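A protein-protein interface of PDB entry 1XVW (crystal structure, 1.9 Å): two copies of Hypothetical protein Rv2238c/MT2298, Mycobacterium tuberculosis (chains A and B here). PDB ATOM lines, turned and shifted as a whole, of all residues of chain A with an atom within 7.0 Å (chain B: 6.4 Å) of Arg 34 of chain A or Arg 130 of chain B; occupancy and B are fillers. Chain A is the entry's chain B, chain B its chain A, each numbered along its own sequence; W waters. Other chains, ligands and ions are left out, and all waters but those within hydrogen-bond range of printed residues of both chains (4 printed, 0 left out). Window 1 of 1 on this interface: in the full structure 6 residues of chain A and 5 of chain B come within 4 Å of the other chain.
The guanidinium group (NE) of Arg 130 of chain A sits at hydrogen-bond distance from the backbone carbonyl oxygen (O) of Ala 36 of chain A, at 3.0 Å. The backbone NH (N) of Gly 35 of chain A is in hydrogen-bond range of the backbone carbonyl oxygen (O) of Arg 130 of chain A, 2.9 Å away. The backbone carbonyl oxygen (O) of Leu 158 of chain B is in hydrogen-bond range of the guanidinium group (NH1) of Arg 130 of chain B (3.2 Å). The backbone carbonyl oxygen (O) of Arg 130 of chain B sits at hydrogen-bond distance from the backbone NH (N) of Gly 35 of chain B, 2.7 Å away. NE of Arg 130 of chain B is in hydrogen-bond range of O of Ala 36 of chain B, at 3.3 Å. NH1 of Arg 130 of chain B sits close to ND2 of Asn 38 of chain B, at 3.4 Å.
Printed residues of chain B within 4 Å of Gly 32 of chain A: Ser 131 (3.4 Å). Of the printed residues of chain B, Arg 34 of chain A touches Arg 34 (3.4 Å), Arg 130 (3.9 Å) and Ser 131 (2.8 Å). Of the printed residues of chain B, Ala 36 of chain A touches Ser 131 (3.5 Å). Printed residues of chain B within 4 Å of Ser 131 of chain A: Arg 34 (3.5 Å). Printed residues of chain A within 4 Å of Arg 34 of chain B: Arg 34 (3.4 Å) and Ser 131 (3.5 Å). Of the printed residues of chain A, Gly 35 of chain B touches Gly 35. Of chain A, only Arg 34 and Gly 35 come within 4 Å of Arg 130 of chain B. The nearest residue of chain A that does not touch Arg 130 of chain B is Ala 36 of chain A (5.2 Å).
The side-chain hydroxyl of Ser 131 of chain B is in hydrogen-bond range of the backbone carbonyl oxygen of Arg 34 of chain A (2.8 Å). The side-chain hydroxyl (OG) of Ser 131 of chain B is in hydrogen-bond range of the backbone carbonyl oxygen (O) of Gly 32 of chain A (3.4 Å). The guanidinium group of Arg 34 of chain B sits at hydrogen-bond distance from the backbone carbonyl oxygen of Ser 131 of chain A, at 3.5 Å.
Among the printed residues, merely in contact across the chains: Arg 34 of chain A with Arg 34 of chain B, Ala 36 of chain A with Ser 131 of chain B, Gly 35 of chain A with Gly 35 of chain B, Gly 35 of chain A with Arg 130 of chain B and Arg 34 of chain A with Arg 130 of chain B.
Arg 34 of chain B touches its own counterpart, Arg 34 of chain A. Arg 34 of chain A touches Ser 131 of chain B, and with the chains exchanged Ser 131 of chain A touches Arg 34 of chain B. Gly 35 of chain A touches its own counterpart, Gly 35 of chain B. Ala 36 of chain A touches Ser 131 of chain B, but with the chains exchanged Ser 131 of chain A does not touch Ala 36 of chain B (10.0 Å). Positions printed for both chains: 31, 33, 34, 35, 36, 37, 39, 128, 129, 130, 131, 132 and 133.
Of the 19 printed residues of chain B, 4 touch a printed residue of chain A. Printed residues of chain B that touch a printed residue of chain A: Arg 34, Gly 35, Arg 130 and Ser 131. Of the 20 printed residues of chain A, 5 touch a printed residue of chain B.
Water W3 lies within hydrogen-bond range of O of Gly 32 of chain A (2.6 Å) and OG of Ser 131 of chain B (2.8 Å). Water W2 bridges O of Arg 31 of chain A (2.7 Å) and O of Ser 131 of chain B (2.7 Å). Water W1 bridges NE of Arg 34 of chain B (2.8 Å) and O of Arg 130 of chain A (3.4 Å). Water W4 lies within hydrogen-bond range of O of Ser 131 of chain A, NH2 of Arg 34 of chain B and NH1 of Arg 34 of chain A.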
ATOM      1  N   THR A  14       5.957   6.057 -17.216  1.00  0.00           N
ATOM      2  CA  THR A  14       5.348   4.778 -16.847  1.00  0.00           C
ATOM      3  C   THR A  14       6.311   4.192 -15.791  1.00  0.00           C
ATOM      4  O   THR A  14       7.517   4.181 -16.022  1.00  0.00           O
ATOM      5  CB  THR A  14       5.351   3.843 -18.052  1.00  0.00           C
ATOM      6  OG1 THR A  14       4.495   4.399 -19.067  1.00  0.00           O
ATOM      7  CG2 THR A  14       4.891   2.432 -17.646  1.00  0.00           C
ATOM      8  N   ALA A  15       5.804   3.744 -14.642  1.00  0.00           N
ATOM      9  CA  ALA A  15       6.666   3.137 -13.611  1.00  0.00           C
ATOM     10  C   ALA A  15       7.020   1.706 -14.050  1.00  0.00           C
ATOM     11  O   ALA A  15       6.120   0.922 -14.390  1.00  0.00           O
ATOM     12  CB  ALA A  15       5.934   3.090 -12.251  1.00  0.00           C
ATOM     13  N   PRO A  16       8.325   1.363 -14.076  1.00  0.00           N
ATOM     14  CA  PRO A  16       8.749   0.017 -14.482  1.00  0.00           C
ATOM     15  C   PRO A  16       8.058  -1.022 -13.610  1.00  0.00           C
ATOM     16  O   PRO A  16       8.074  -0.921 -12.380  1.00  0.00           O
ATOM     17  CB  PRO A  16      10.253   0.030 -14.255  1.00  0.00           C
ATOM     18  CG  PRO A  16      10.623   1.476 -14.591  1.00  0.00           C
ATOM     19  CD  PRO A  16       9.484   2.264 -13.919  1.00  0.00           C
ATOM     20  N   ASP A  17       7.435  -1.999 -14.256  1.00  0.00           N
ATOM     21  CA  ASP A  17       6.715  -3.041 -13.525  1.00  0.00           C
ATOM     22  C   ASP A  17       7.722  -4.034 -12.938  1.00  0.00           C
ATOM     23  O   ASP A  17       8.881  -4.084 -13.377  1.00  0.00           O
ATOM     24  CB  ASP A  17       5.731  -3.708 -14.479  1.00  0.00           C
ATOM     25  CG  ASP A  17       4.854  -4.754 -13.803  1.00  0.00           C
ATOM     26  OD1 ASP A  17       4.671  -4.731 -12.558  1.00  0.00           O
ATOM     27  OD2 ASP A  17       4.329  -5.613 -14.545  1.00  0.00           O
ATOM     28  N   THR A  29       3.500  -7.923  -7.165  1.00  0.00           N
ATOM     29  CA  THR A  29       3.691  -7.404  -8.514  1.00  0.00           C
ATOM     30  C   THR A  29       3.143  -5.993  -8.570  1.00  0.00           C
ATOM     31  O   THR A  29       2.036  -5.762  -8.134  1.00  0.00           O
ATOM     32  CB  THR A  29       2.940  -8.298  -9.520  1.00  0.00           C
ATOM     33  OG1 THR A  29       3.534  -9.600  -9.494  1.00  0.00           O
ATOM     34  CG2 THR A  29       3.035  -7.744 -10.928  1.00  0.00           C
ATOM     35  N   LEU A  30       3.910  -5.057  -9.117  1.00  0.00           N
ATOM     36  CA  LEU A  30       3.433  -3.687  -9.165  1.00  0.00           C
ATOM     37  C   LEU A  30       2.142  -3.511  -9.959  1.00  0.00           C
ATOM     38  O   LEU A  30       1.217  -2.847  -9.502  1.00  0.00           O
ATOM     39  CB  LEU A  30       4.501  -2.763  -9.762  1.00  0.00           C
ATOM     40  CG  LEU A  30       4.068  -1.294  -9.788  1.00  0.00           C
ATOM     41  CD1 LEU A  30       3.805  -0.769  -8.362  1.00  0.00           C
ATOM     42  CD2 LEU A  30       5.159  -0.482 -10.459  1.00  0.00           C
ATOM     43  N   ARG A  31       2.074  -4.099 -11.152  1.00  0.00           N
ATOM     44  CA  ARG A  31       0.891  -3.916 -11.983  1.00  0.00           C
ATOM     45  C   ARG A  31      -0.393  -4.442 -11.339  1.00  0.00           C
ATOM     46  O   ARG A  31      -1.488  -4.087 -11.771  1.00  0.00           O
ATOM     47  CB  ARG A  31       1.097  -4.563 -13.371  1.00  0.00           C
ATOM     48  CG  ARG A  31       1.185  -6.087 -13.334  1.00  0.00           C
ATOM     49  CD  ARG A  31       1.264  -6.688 -14.742  1.00  0.00           C
ATOM     50  NE  ARG A  31       1.349  -8.152 -14.721  1.00  0.00           N
ATOM     51  CZ  ARG A  31       2.478  -8.843 -14.548  1.00  0.00           C
ATOM     52  NH1 ARG A  31       3.641  -8.214 -14.380  1.00  0.00           N
ATOM     53  NH2 ARG A  31       2.450 -10.167 -14.541  1.00  0.00           N
ATOM     54  N   GLY A  32      -0.273  -5.273 -10.300  1.00  0.00           N
ATOM     55  CA  GLY A  32      -1.474  -5.790  -9.649  1.00  0.00           C
ATOM     56  C   GLY A  32      -2.321  -4.713  -8.977  1.00  0.00           C
ATOM     57  O   GLY A  32      -3.506  -4.919  -8.710  1.00  0.00           O
ATOM     58  N   TYR A  33      -1.729  -3.547  -8.693  1.00  0.00           N
ATOM     59  CA  TYR A  33      -2.481  -2.456  -8.054  1.00  0.00           C
ATOM     60  C   TYR A  33      -3.215  -1.534  -9.033  1.00  0.00           C
ATOM     61  O   TYR A  33      -4.060  -0.730  -8.626  1.00  0.00           O
ATOM     62  CB  TYR A  33      -1.531  -1.594  -7.195  1.00  0.00           C
ATOM     63  CG  TYR A  33      -0.948  -2.368  -6.025  1.00  0.00           C
ATOM     64  CD1 TYR A  33       0.303  -2.967  -6.120  1.00  0.00           C
ATOM     65  CD2 TYR A  33      -1.654  -2.498  -4.835  1.00  0.00           C
ATOM     66  CE1 TYR A  33       0.848  -3.687  -5.045  1.00  0.00           C
ATOM     67  CE2 TYR A  33      -1.124  -3.207  -3.750  1.00  0.00           C
ATOM     68  CZ  TYR A  33       0.127  -3.798  -3.864  1.00  0.00           C
ATOM     69  OH  TYR A  33       0.672  -4.494  -2.807  1.00  0.00           O
ATOM     70  N   ARG A  34      -2.867  -1.619 -10.310  1.00  0.00           N
ATOM     71  CA  ARG A  34      -3.484  -0.764 -11.314  1.00  0.00           C
ATOM     72  C   ARG A  34      -5.000  -0.891 -11.269  1.00  0.00           C
ATOM     73  O   ARG A  34      -5.547  -1.988 -11.060  1.00  0.00           O
ATOM     74  CB  ARG A  34      -2.972  -1.112 -12.712  1.00  0.00           C
ATOM     75  CG  ARG A  34      -1.491  -0.804 -12.907  1.00  0.00           C
ATOM     76  CD  ARG A  34      -1.015  -1.254 -14.271  1.00  0.00           C
ATOM     77  NE  ARG A  34       0.416  -1.050 -14.469  1.00  0.00           N
ATOM     78  CZ  ARG A  34       1.084  -1.515 -15.525  1.00  0.00           C
ATOM     79  NH1 ARG A  34       0.442  -2.207 -16.463  1.00  0.00           N
ATOM     80  NH2 ARG A  34       2.388  -1.301 -15.650  1.00  0.00           N
ATOM     81  N   GLY A  35      -5.668   0.239 -11.455  1.00  0.00           N
ATOM     82  CA  GLY A  35      -7.119   0.251 -11.427  1.00  0.00           C
ATOM     83  C   GLY A  35      -7.706   0.069 -10.038  1.00  0.00           C
ATOM     84  O   GLY A  35      -8.933  -0.083  -9.908  1.00  0.00           O
ATOM     85  N   ALA A  36      -6.863   0.083  -8.998  1.00  0.00           N
ATOM     86  CA  ALA A  36      -7.352  -0.108  -7.633  1.00  0.00           C
ATOM     87  C   ALA A  36      -6.741   0.826  -6.582  1.00  0.00           C
ATOM     88  O   ALA A  36      -7.461   1.465  -5.819  1.00  0.00           O
ATOM     89  CB  ALA A  36      -7.129  -1.569  -7.185  1.00  0.00           C
ATOM     90  N   LYS A  37      -5.417   0.894  -6.535  1.00  0.00           N
ATOM     91  CA  LYS A  37      -4.771   1.734  -5.536  1.00  0.00           C
ATOM     92  C   LYS A  37      -3.597   2.524  -6.057  1.00  0.00           C
ATOM     93  O   LYS A  37      -2.979   2.130  -7.031  1.00  0.00           O
ATOM     94  CB  LYS A  37      -4.270   0.870  -4.379  1.00  0.00           C
ATOM     95  CG  LYS A  37      -5.393   0.176  -3.625  1.00  0.00           C
ATOM     96  CD  LYS A  37      -4.878  -0.610  -2.429  1.00  0.00           C
ATOM     97  CE  LYS A  37      -6.054  -1.222  -1.628  1.00  0.00           C
ATOM     98  NZ  LYS A  37      -5.569  -2.094  -0.520  1.00  0.00           N
ATOM     99  N   VAL A  39       0.168   3.636  -5.447  1.00  0.00           N
ATOM    100  CA  VAL A  39       1.214   2.922  -4.729  1.00  0.00           C
ATOM    101  C   VAL A  39       2.421   3.769  -4.366  1.00  0.00           C
ATOM    102  O   VAL A  39       3.005   4.416  -5.235  1.00  0.00           O
ATOM    103  CB  VAL A  39       1.710   1.690  -5.571  1.00  0.00           C
ATOM    104  CG1 VAL A  39       2.786   0.904  -4.797  1.00  0.00           C
ATOM    105  CG2 VAL A  39       0.513   0.750  -5.904  1.00  0.00           C
ATOM    106  N   VAL A 128       2.916   5.881  -7.603  1.00  0.00           N
ATOM    107  CA  VAL A 128       2.435   5.365  -8.890  1.00  0.00           C
ATOM    108  C   VAL A 128       0.899   5.425  -8.839  1.00  0.00           C
ATOM    109  O   VAL A 128       0.292   4.882  -7.909  1.00  0.00           O
ATOM    110  CB  VAL A 128       2.931   3.884  -9.099  1.00  0.00           C
ATOM    111  CG1 VAL A 128       2.484   3.333 -10.455  1.00  0.00           C
ATOM    112  CG2 VAL A 128       4.482   3.848  -9.026  1.00  0.00           C
ATOM    113  N   ASP A 129       0.263   6.096  -9.807  1.00  0.00           N
ATOM    114  CA  ASP A 129      -1.187   6.184  -9.756  1.00  0.00           C
ATOM    115  C   ASP A 129      -1.869   4.928 -10.304  1.00  0.00           C
ATOM    116  O   ASP A 129      -1.196   3.959 -10.624  1.00  0.00           O
ATOM    117  CB  ASP A 129      -1.710   7.469 -10.441  1.00  0.00           C
ATOM    118  CG  ASP A 129      -1.525   7.493 -11.974  1.00  0.00           C
ATOM    119  OD1 ASP A 129      -1.327   6.438 -12.621  1.00  0.00           O
ATOM    120  OD2 ASP A 129      -1.611   8.622 -12.542  1.00  0.00           O
ATOM    121  N   ARG A 130      -3.198   4.933 -10.361  1.00  0.00           N
ATOM    122  CA  ARG A 130      -3.958   3.776 -10.838  1.00  0.00           C
ATOM    123  C   ARG A 130      -3.762   3.432 -12.309  1.00  0.00           C
ATOM    124  O   ARG A 130      -4.150   2.342 -12.747  1.00  0.00           O
ATOM    125  CB  ARG A 130      -5.447   3.979 -10.538  1.00  0.00           C
ATOM    126  CG  ARG A 130      -5.708   4.006  -9.061  1.00  0.00           C
ATOM    127  CD  ARG A 130      -7.177   4.158  -8.697  1.00  0.00           C
ATOM    128  NE  ARG A 130      -7.285   4.152  -7.234  1.00  0.00           N
ATOM    129  CZ  ARG A 130      -7.182   5.230  -6.452  1.00  0.00           C
ATOM    130  NH1 ARG A 130      -6.980   6.435  -6.986  1.00  0.00           N
ATOM    131  NH2 ARG A 130      -7.261   5.099  -5.128  1.00  0.00           N
ATOM    132  N   SER A 131      -3.170   4.351 -13.079  1.00  0.00           N
ATOM    133  CA  SER A 131      -2.901   4.086 -14.492  1.00  0.00           C
ATOM    134  C   SER A 131      -1.476   3.577 -14.724  1.00  0.00           C
ATOM    135  O   SER A 131      -1.098   3.262 -15.853  1.00  0.00           O
ATOM    136  CB  SER A 131      -3.108   5.350 -15.328  1.00  0.00           C
ATOM    137  OG  SER A 131      -4.453   5.747 -15.240  1.00  0.00           O
ATOM    138  N   GLY A 132      -0.689   3.510 -13.648  1.00  0.00           N
ATOM    139  CA  GLY A 132       0.684   3.047 -13.752  1.00  0.00           C
ATOM    140  C   GLY A 132       1.694   4.161 -14.026  1.00  0.00           C
ATOM    141  O   GLY A 132       2.853   3.888 -14.344  1.00  0.00           O
ATOM    142  N   ILE A 133       1.265   5.409 -13.888  1.00  0.00           N
ATOM    143  CA  ILE A 133       2.124   6.566 -14.169  1.00  0.00           C
ATOM    144  C   ILE A 133       2.685   7.164 -12.874  1.00  0.00           C
ATOM    145  O   ILE A 133       1.967   7.268 -11.877  1.00  0.00           O
ATOM    146  CB  ILE A 133       1.310   7.660 -14.900  1.00  0.00           C
ATOM    147  CG1 ILE A 133       0.913   7.176 -16.311  1.00  0.00           C
ATOM    148  CG2 ILE A 133       2.084   8.984 -14.923  1.00  0.00           C
ATOM    149  CD1 ILE A 133       2.076   6.917 -17.270  1.00  0.00           C
ATOM    150  N   ARG B  31      -8.460  -3.673 -21.872  1.00  0.00           N
ATOM    151  CA  ARG B  31      -7.861  -2.600 -21.064  1.00  0.00           C
ATOM    152  C   ARG B  31      -8.871  -1.466 -20.812  1.00  0.00           C
ATOM    153  O   ARG B  31      -8.855  -0.799 -19.765  1.00  0.00           O
ATOM    154  CB  ARG B  31      -6.611  -2.087 -21.810  1.00  0.00           C
ATOM    155  CG  ARG B  31      -5.878  -0.876 -21.215  1.00  0.00           C
ATOM    156  CD  ARG B  31      -5.299  -1.174 -19.833  1.00  0.00           C
ATOM    157  NE  ARG B  31      -4.132  -2.061 -19.845  1.00  0.00           N
ATOM    158  CZ  ARG B  31      -2.884  -1.665 -20.104  1.00  0.00           C
ATOM    159  NH1 ARG B  31      -2.621  -0.385 -20.389  1.00  0.00           N
ATOM    160  NH2 ARG B  31      -1.894  -2.539 -20.032  1.00  0.00           N
ATOM    161  N   TYR B  33     -11.745  -1.504 -19.804  1.00  0.00           N
ATOM    162  CA  TYR B  33     -12.533  -1.695 -18.583  1.00  0.00           C
ATOM    163  C   TYR B  33     -11.738  -1.549 -17.294  1.00  0.00           C
ATOM    164  O   TYR B  33     -12.314  -1.472 -16.202  1.00  0.00           O
ATOM    165  CB  TYR B  33     -13.188  -3.088 -18.564  1.00  0.00           C
ATOM    166  CG  TYR B  33     -14.147  -3.320 -19.716  1.00  0.00           C
ATOM    167  CD1 TYR B  33     -13.722  -3.957 -20.879  1.00  0.00           C
ATOM    168  CD2 TYR B  33     -15.471  -2.872 -19.654  1.00  0.00           C
ATOM    169  CE1 TYR B  33     -14.593  -4.144 -21.976  1.00  0.00           C
ATOM    170  CE2 TYR B  33     -16.357  -3.056 -20.754  1.00  0.00           C
ATOM    171  CZ  TYR B  33     -15.902  -3.686 -21.897  1.00  0.00           C
ATOM    172  OH  TYR B  33     -16.740  -3.866 -22.982  1.00  0.00           O
ATOM    173  N   ARG B  34     -10.419  -1.529 -17.411  1.00  0.00           N
ATOM    174  CA  ARG B  34      -9.581  -1.450 -16.225  1.00  0.00           C
ATOM    175  C   ARG B  34      -9.954  -0.224 -15.394  1.00  0.00           C
ATOM    176  O   ARG B  34     -10.189   0.871 -15.932  1.00  0.00           O
ATOM    177  CB  ARG B  34      -8.101  -1.431 -16.639  1.00  0.00           C
ATOM    178  CG  ARG B  34      -7.089  -1.776 -15.516  1.00  0.00           C
ATOM    179  CD  ARG B  34      -5.606  -1.769 -15.997  1.00  0.00           C
ATOM    180  NE  ARG B  34      -5.105  -0.417 -16.315  1.00  0.00           N
ATOM    181  CZ  ARG B  34      -3.878  -0.141 -16.774  1.00  0.00           C
ATOM    182  NH1 ARG B  34      -3.001  -1.110 -16.982  1.00  0.00           N
ATOM    183  NH2 ARG B  34      -3.529   1.114 -17.039  1.00  0.00           N
ATOM    184  N   GLY B  35     -10.049  -0.429 -14.083  1.00  0.00           N
ATOM    185  CA  GLY B  35     -10.400   0.642 -13.172  1.00  0.00           C
ATOM    186  C   GLY B  35     -11.888   0.920 -13.107  1.00  0.00           C
ATOM    187  O   GLY B  35     -12.331   1.679 -12.246  1.00  0.00           O
ATOM    188  N   ALA B  36     -12.674   0.279 -13.973  1.00  0.00           N
ATOM    189  CA  ALA B  36     -14.115   0.553 -14.017  1.00  0.00           C
ATOM    190  C   ALA B  36     -15.068  -0.635 -13.808  1.00  0.00           C
ATOM    191  O   ALA B  36     -16.029  -0.538 -13.037  1.00  0.00           O
ATOM    192  CB  ALA B  36     -14.442   1.236 -15.346  1.00  0.00           C
ATOM    193  N   LYS B  37     -14.808  -1.757 -14.480  1.00  0.00           N
ATOM    194  CA  LYS B  37     -15.709  -2.905 -14.341  1.00  0.00           C
ATOM    195  C   LYS B  37     -14.999  -4.234 -14.316  1.00  0.00           C
ATOM    196  O   LYS B  37     -13.903  -4.378 -14.859  1.00  0.00           O
ATOM    197  CB  LYS B  37     -16.690  -2.955 -15.526  1.00  0.00           C
ATOM    198  CG  LYS B  37     -17.594  -1.727 -15.653  1.00  0.00           C
ATOM    199  CD  LYS B  37     -18.458  -1.795 -16.894  1.00  0.00           C
ATOM    200  CE  LYS B  37     -19.330  -0.542 -16.976  1.00  0.00           C
ATOM    201  NZ  LYS B  37     -20.489  -0.709 -17.907  1.00  0.00           N
ATOM    202  N   ASN B  38     -15.645  -5.218 -13.708  1.00  0.00           N
ATOM    203  CA  ASN B  38     -15.080  -6.561 -13.713  1.00  0.00           C
ATOM    204  C   ASN B  38     -15.562  -7.092 -15.060  1.00  0.00           C
ATOM    205  O   ASN B  38     -16.621  -6.671 -15.532  1.00  0.00           O
ATOM    206  CB  ASN B  38     -15.671  -7.372 -12.562  1.00  0.00           C
ATOM    207  CG  ASN B  38     -15.231  -6.845 -11.230  1.00  0.00           C
ATOM    208  OD1 ASN B  38     -14.035  -6.717 -10.980  1.00  0.00           O
ATOM    209  ND2 ASN B  38     -16.181  -6.527 -10.371  1.00  0.00           N
ATOM    210  N   VAL B  39     -14.805  -7.977 -15.694  1.00  0.00           N
ATOM    211  CA  VAL B  39     -15.216  -8.466 -17.010  1.00  0.00           C
ATOM    212  C   VAL B  39     -15.325  -9.987 -17.069  1.00  0.00           C
ATOM    213  O   VAL B  39     -14.402 -10.718 -16.680  1.00  0.00           O
ATOM    214  CB  VAL B  39     -14.230  -7.980 -18.116  1.00  0.00           C
ATOM    215  CG1 VAL B  39     -14.765  -8.342 -19.514  1.00  0.00           C
ATOM    216  CG2 VAL B  39     -14.030  -6.447 -18.011  1.00  0.00           C
ATOM    217  N   ASP B  69     -23.299  -1.323 -14.034  1.00  0.00           N
ATOM    218  CA  ASP B  69     -22.241  -0.385 -13.709  1.00  0.00           C
ATOM    219  C   ASP B  69     -21.002  -1.072 -13.138  1.00  0.00           C
ATOM    220  O   ASP B  69     -19.907  -0.521 -13.194  1.00  0.00           O
ATOM    221  CB  ASP B  69     -22.753   0.670 -12.721  1.00  0.00           C
ATOM    222  CG  ASP B  69     -23.819   1.561 -13.330  1.00  0.00           C
ATOM    223  OD1 ASP B  69     -23.602   2.056 -14.458  1.00  0.00           O
ATOM    224  OD2 ASP B  69     -24.871   1.766 -12.685  1.00  0.00           O
ATOM    225  N   ASP B  70     -21.169  -2.286 -12.620  1.00  0.00           N
ATOM    226  CA  ASP B  70     -20.056  -3.010 -12.019  1.00  0.00           C
ATOM    227  C   ASP B  70     -19.399  -4.046 -12.934  1.00  0.00           C
ATOM    228  O   ASP B  70     -18.298  -4.488 -12.659  1.00  0.00           O
ATOM    229  CB  ASP B  70     -20.522  -3.718 -10.751  1.00  0.00           C
ATOM    230  CG  ASP B  70     -21.100  -2.760  -9.727  1.00  0.00           C
ATOM    231  OD1 ASP B  70     -20.597  -1.619  -9.641  1.00  0.00           O
ATOM    232  OD2 ASP B  70     -22.045  -3.160  -9.005  1.00  0.00           O
ATOM    233  N   SER B  71     -20.074  -4.447 -14.004  1.00  0.00           N
ATOM    234  CA  SER B  71     -19.489  -5.447 -14.870  1.00  0.00           C
ATOM    235  C   SER B  71     -19.979  -5.487 -16.296  1.00  0.00           C
ATOM    236  O   SER B  71     -20.998  -4.878 -16.643  1.00  0.00           O
ATOM    237  CB  SER B  71     -19.634  -6.833 -14.244  1.00  0.00           C
ATOM    238  OG  SER B  71     -20.905  -7.024 -13.670  1.00  0.00           O
ATOM    239  N   VAL B 128     -12.293 -11.169 -15.033  1.00  0.00           N
ATOM    240  CA  VAL B 128     -11.109 -10.339 -14.884  1.00  0.00           C
ATOM    241  C   VAL B 128     -11.535  -9.188 -13.972  1.00  0.00           C
ATOM    242  O   VAL B 128     -12.595  -8.604 -14.192  1.00  0.00           O
ATOM    243  CB  VAL B 128     -10.653  -9.814 -16.266  1.00  0.00           C
ATOM    244  CG1 VAL B 128      -9.368  -8.971 -16.122  1.00  0.00           C
ATOM    245  CG2 VAL B 128     -10.422 -10.999 -17.209  1.00  0.00           C
ATOM    246  N   ASP B 129     -10.744  -8.860 -12.946  1.00  0.00           N
ATOM    247  CA  ASP B 129     -11.164  -7.781 -12.053  1.00  0.00           C
ATOM    248  C   ASP B 129     -10.774  -6.404 -12.605  1.00  0.00           C
ATOM    249  O   ASP B 129     -10.245  -6.313 -13.708  1.00  0.00           O
ATOM    250  CB  ASP B 129     -10.607  -7.994 -10.618  1.00  0.00           C
ATOM    251  CG  ASP B 129      -9.092  -7.903 -10.524  1.00  0.00           C
ATOM    252  OD1 ASP B 129      -8.427  -7.403 -11.466  1.00  0.00           O
ATOM    253  OD2 ASP B 129      -8.551  -8.328  -9.466  1.00  0.00           O
ATOM    254  N   ARG B 130     -11.065  -5.350 -11.841  1.00  0.00           N
ATOM    255  CA  ARG B 130     -10.757  -3.972 -12.247  1.00  0.00           C
ATOM    256  C   ARG B 130      -9.271  -3.675 -12.379  1.00  0.00           C
ATOM    257  O   ARG B 130      -8.889  -2.629 -12.937  1.00  0.00           O
ATOM    258  CB  ARG B 130     -11.393  -2.980 -11.281  1.00  0.00           C
ATOM    259  CG  ARG B 130     -12.902  -2.955 -11.333  1.00  0.00           C
ATOM    260  CD  ARG B 130     -13.478  -2.112 -10.193  1.00  0.00           C
ATOM    261  NE  ARG B 130     -14.932  -2.031 -10.311  1.00  0.00           N
ATOM    262  CZ  ARG B 130     -15.795  -2.786  -9.630  1.00  0.00           C
ATOM    263  NH1 ARG B 130     -15.356  -3.686  -8.749  1.00  0.00           N
ATOM    264  NH2 ARG B 130     -17.101  -2.671  -9.865  1.00  0.00           N
ATOM    265  N   SER B 131      -8.432  -4.587 -11.888  1.00  0.00           N
ATOM    266  CA  SER B 131      -6.974  -4.452 -12.014  1.00  0.00           C
ATOM    267  C   SER B 131      -6.430  -5.279 -13.195  1.00  0.00           C
ATOM    268  O   SER B 131      -5.214  -5.324 -13.440  1.00  0.00           O
ATOM    269  CB  SER B 131      -6.265  -4.895 -10.720  1.00  0.00           C
ATOM    270  OG  SER B 131      -6.665  -4.078  -9.637  1.00  0.00           O
ATOM    271  N   GLY B 132      -7.332  -5.926 -13.936  1.00  0.00           N
ATOM    272  CA  GLY B 132      -6.899  -6.736 -15.059  1.00  0.00           C
ATOM    273  C   GLY B 132      -6.372  -8.109 -14.639  1.00  0.00           C
ATOM    274  O   GLY B 132      -5.690  -8.784 -15.408  1.00  0.00           O
ATOM    275  N   ILE B 133      -6.705  -8.527 -13.423  1.00  0.00           N
ATOM    276  CA  ILE B 133      -6.230  -9.809 -12.922  1.00  0.00           C
ATOM    277  C   ILE B 133      -7.303 -10.887 -13.037  1.00  0.00           C
ATOM    278  O   ILE B 133      -8.460 -10.628 -12.784  1.00  0.00           O
ATOM    279  CB  ILE B 133      -5.832  -9.693 -11.435  1.00  0.00           C
ATOM    280  CG1 ILE B 133      -4.752  -8.616 -11.259  1.00  0.00           C
ATOM    281  CG2 ILE B 133      -5.381 -11.076 -10.906  1.00  0.00           C
ATOM    282  CD1 ILE B 133      -3.441  -8.909 -11.981  1.00  0.00           C
ATOM    283  N   LEU B 158     -16.685  -9.882  -6.366  1.00  0.00           N
ATOM    284  CA  LEU B 158     -15.783  -8.780  -6.697  1.00  0.00           C
ATOM    285  C   LEU B 158     -16.412  -7.402  -6.591  1.00  0.00           C
ATOM    286  O   LEU B 158     -15.909  -6.433  -7.172  1.00  0.00           O
ATOM    287  CB  LEU B 158     -15.239  -8.967  -8.115  1.00  0.00           C
ATOM    288  CG  LEU B 158     -14.502 -10.285  -8.366  1.00  0.00           C
ATOM    289  CD1 LEU B 158     -14.114 -10.401  -9.856  1.00  0.00           C
ATOM    290  CD2 LEU B 158     -13.270 -10.350  -7.451  1.00  0.00           C
ATOM    291  N   THR B 159     -17.515  -7.324  -5.857  1.00  0.00           N
ATOM    292  CA  THR B 159     -18.226  -6.064  -5.676  1.00  0.00           C
ATOM    293  C   THR B 159     -18.598  -5.827  -4.210  1.00  0.00           C
ATOM    294  O   THR B 159     -17.732  -5.467  -3.403  1.00  0.00           O
ATOM    295  CB  THR B 159     -19.512  -6.017  -6.565  1.00  0.00           C
ATOM    296  OG1 THR B 159     -20.252  -4.821  -6.278  1.00  0.00           O
ATOM    297  CG2 THR B 159     -20.394  -7.245  -6.333  1.00  0.00           C
HETATM  298  O   HOH W   1      -6.428   1.799 -15.147  1.00  0.00           O
HETATM  299  O   HOH W   2      -2.514  -5.292 -13.907  1.00  0.00           O
HETATM  300  O   HOH W   3      -5.629  -5.190  -7.318  1.00  0.00           O
HETATM  301  O   HOH W   4      -0.200   0.927 -17.667  1.00  0.00           O
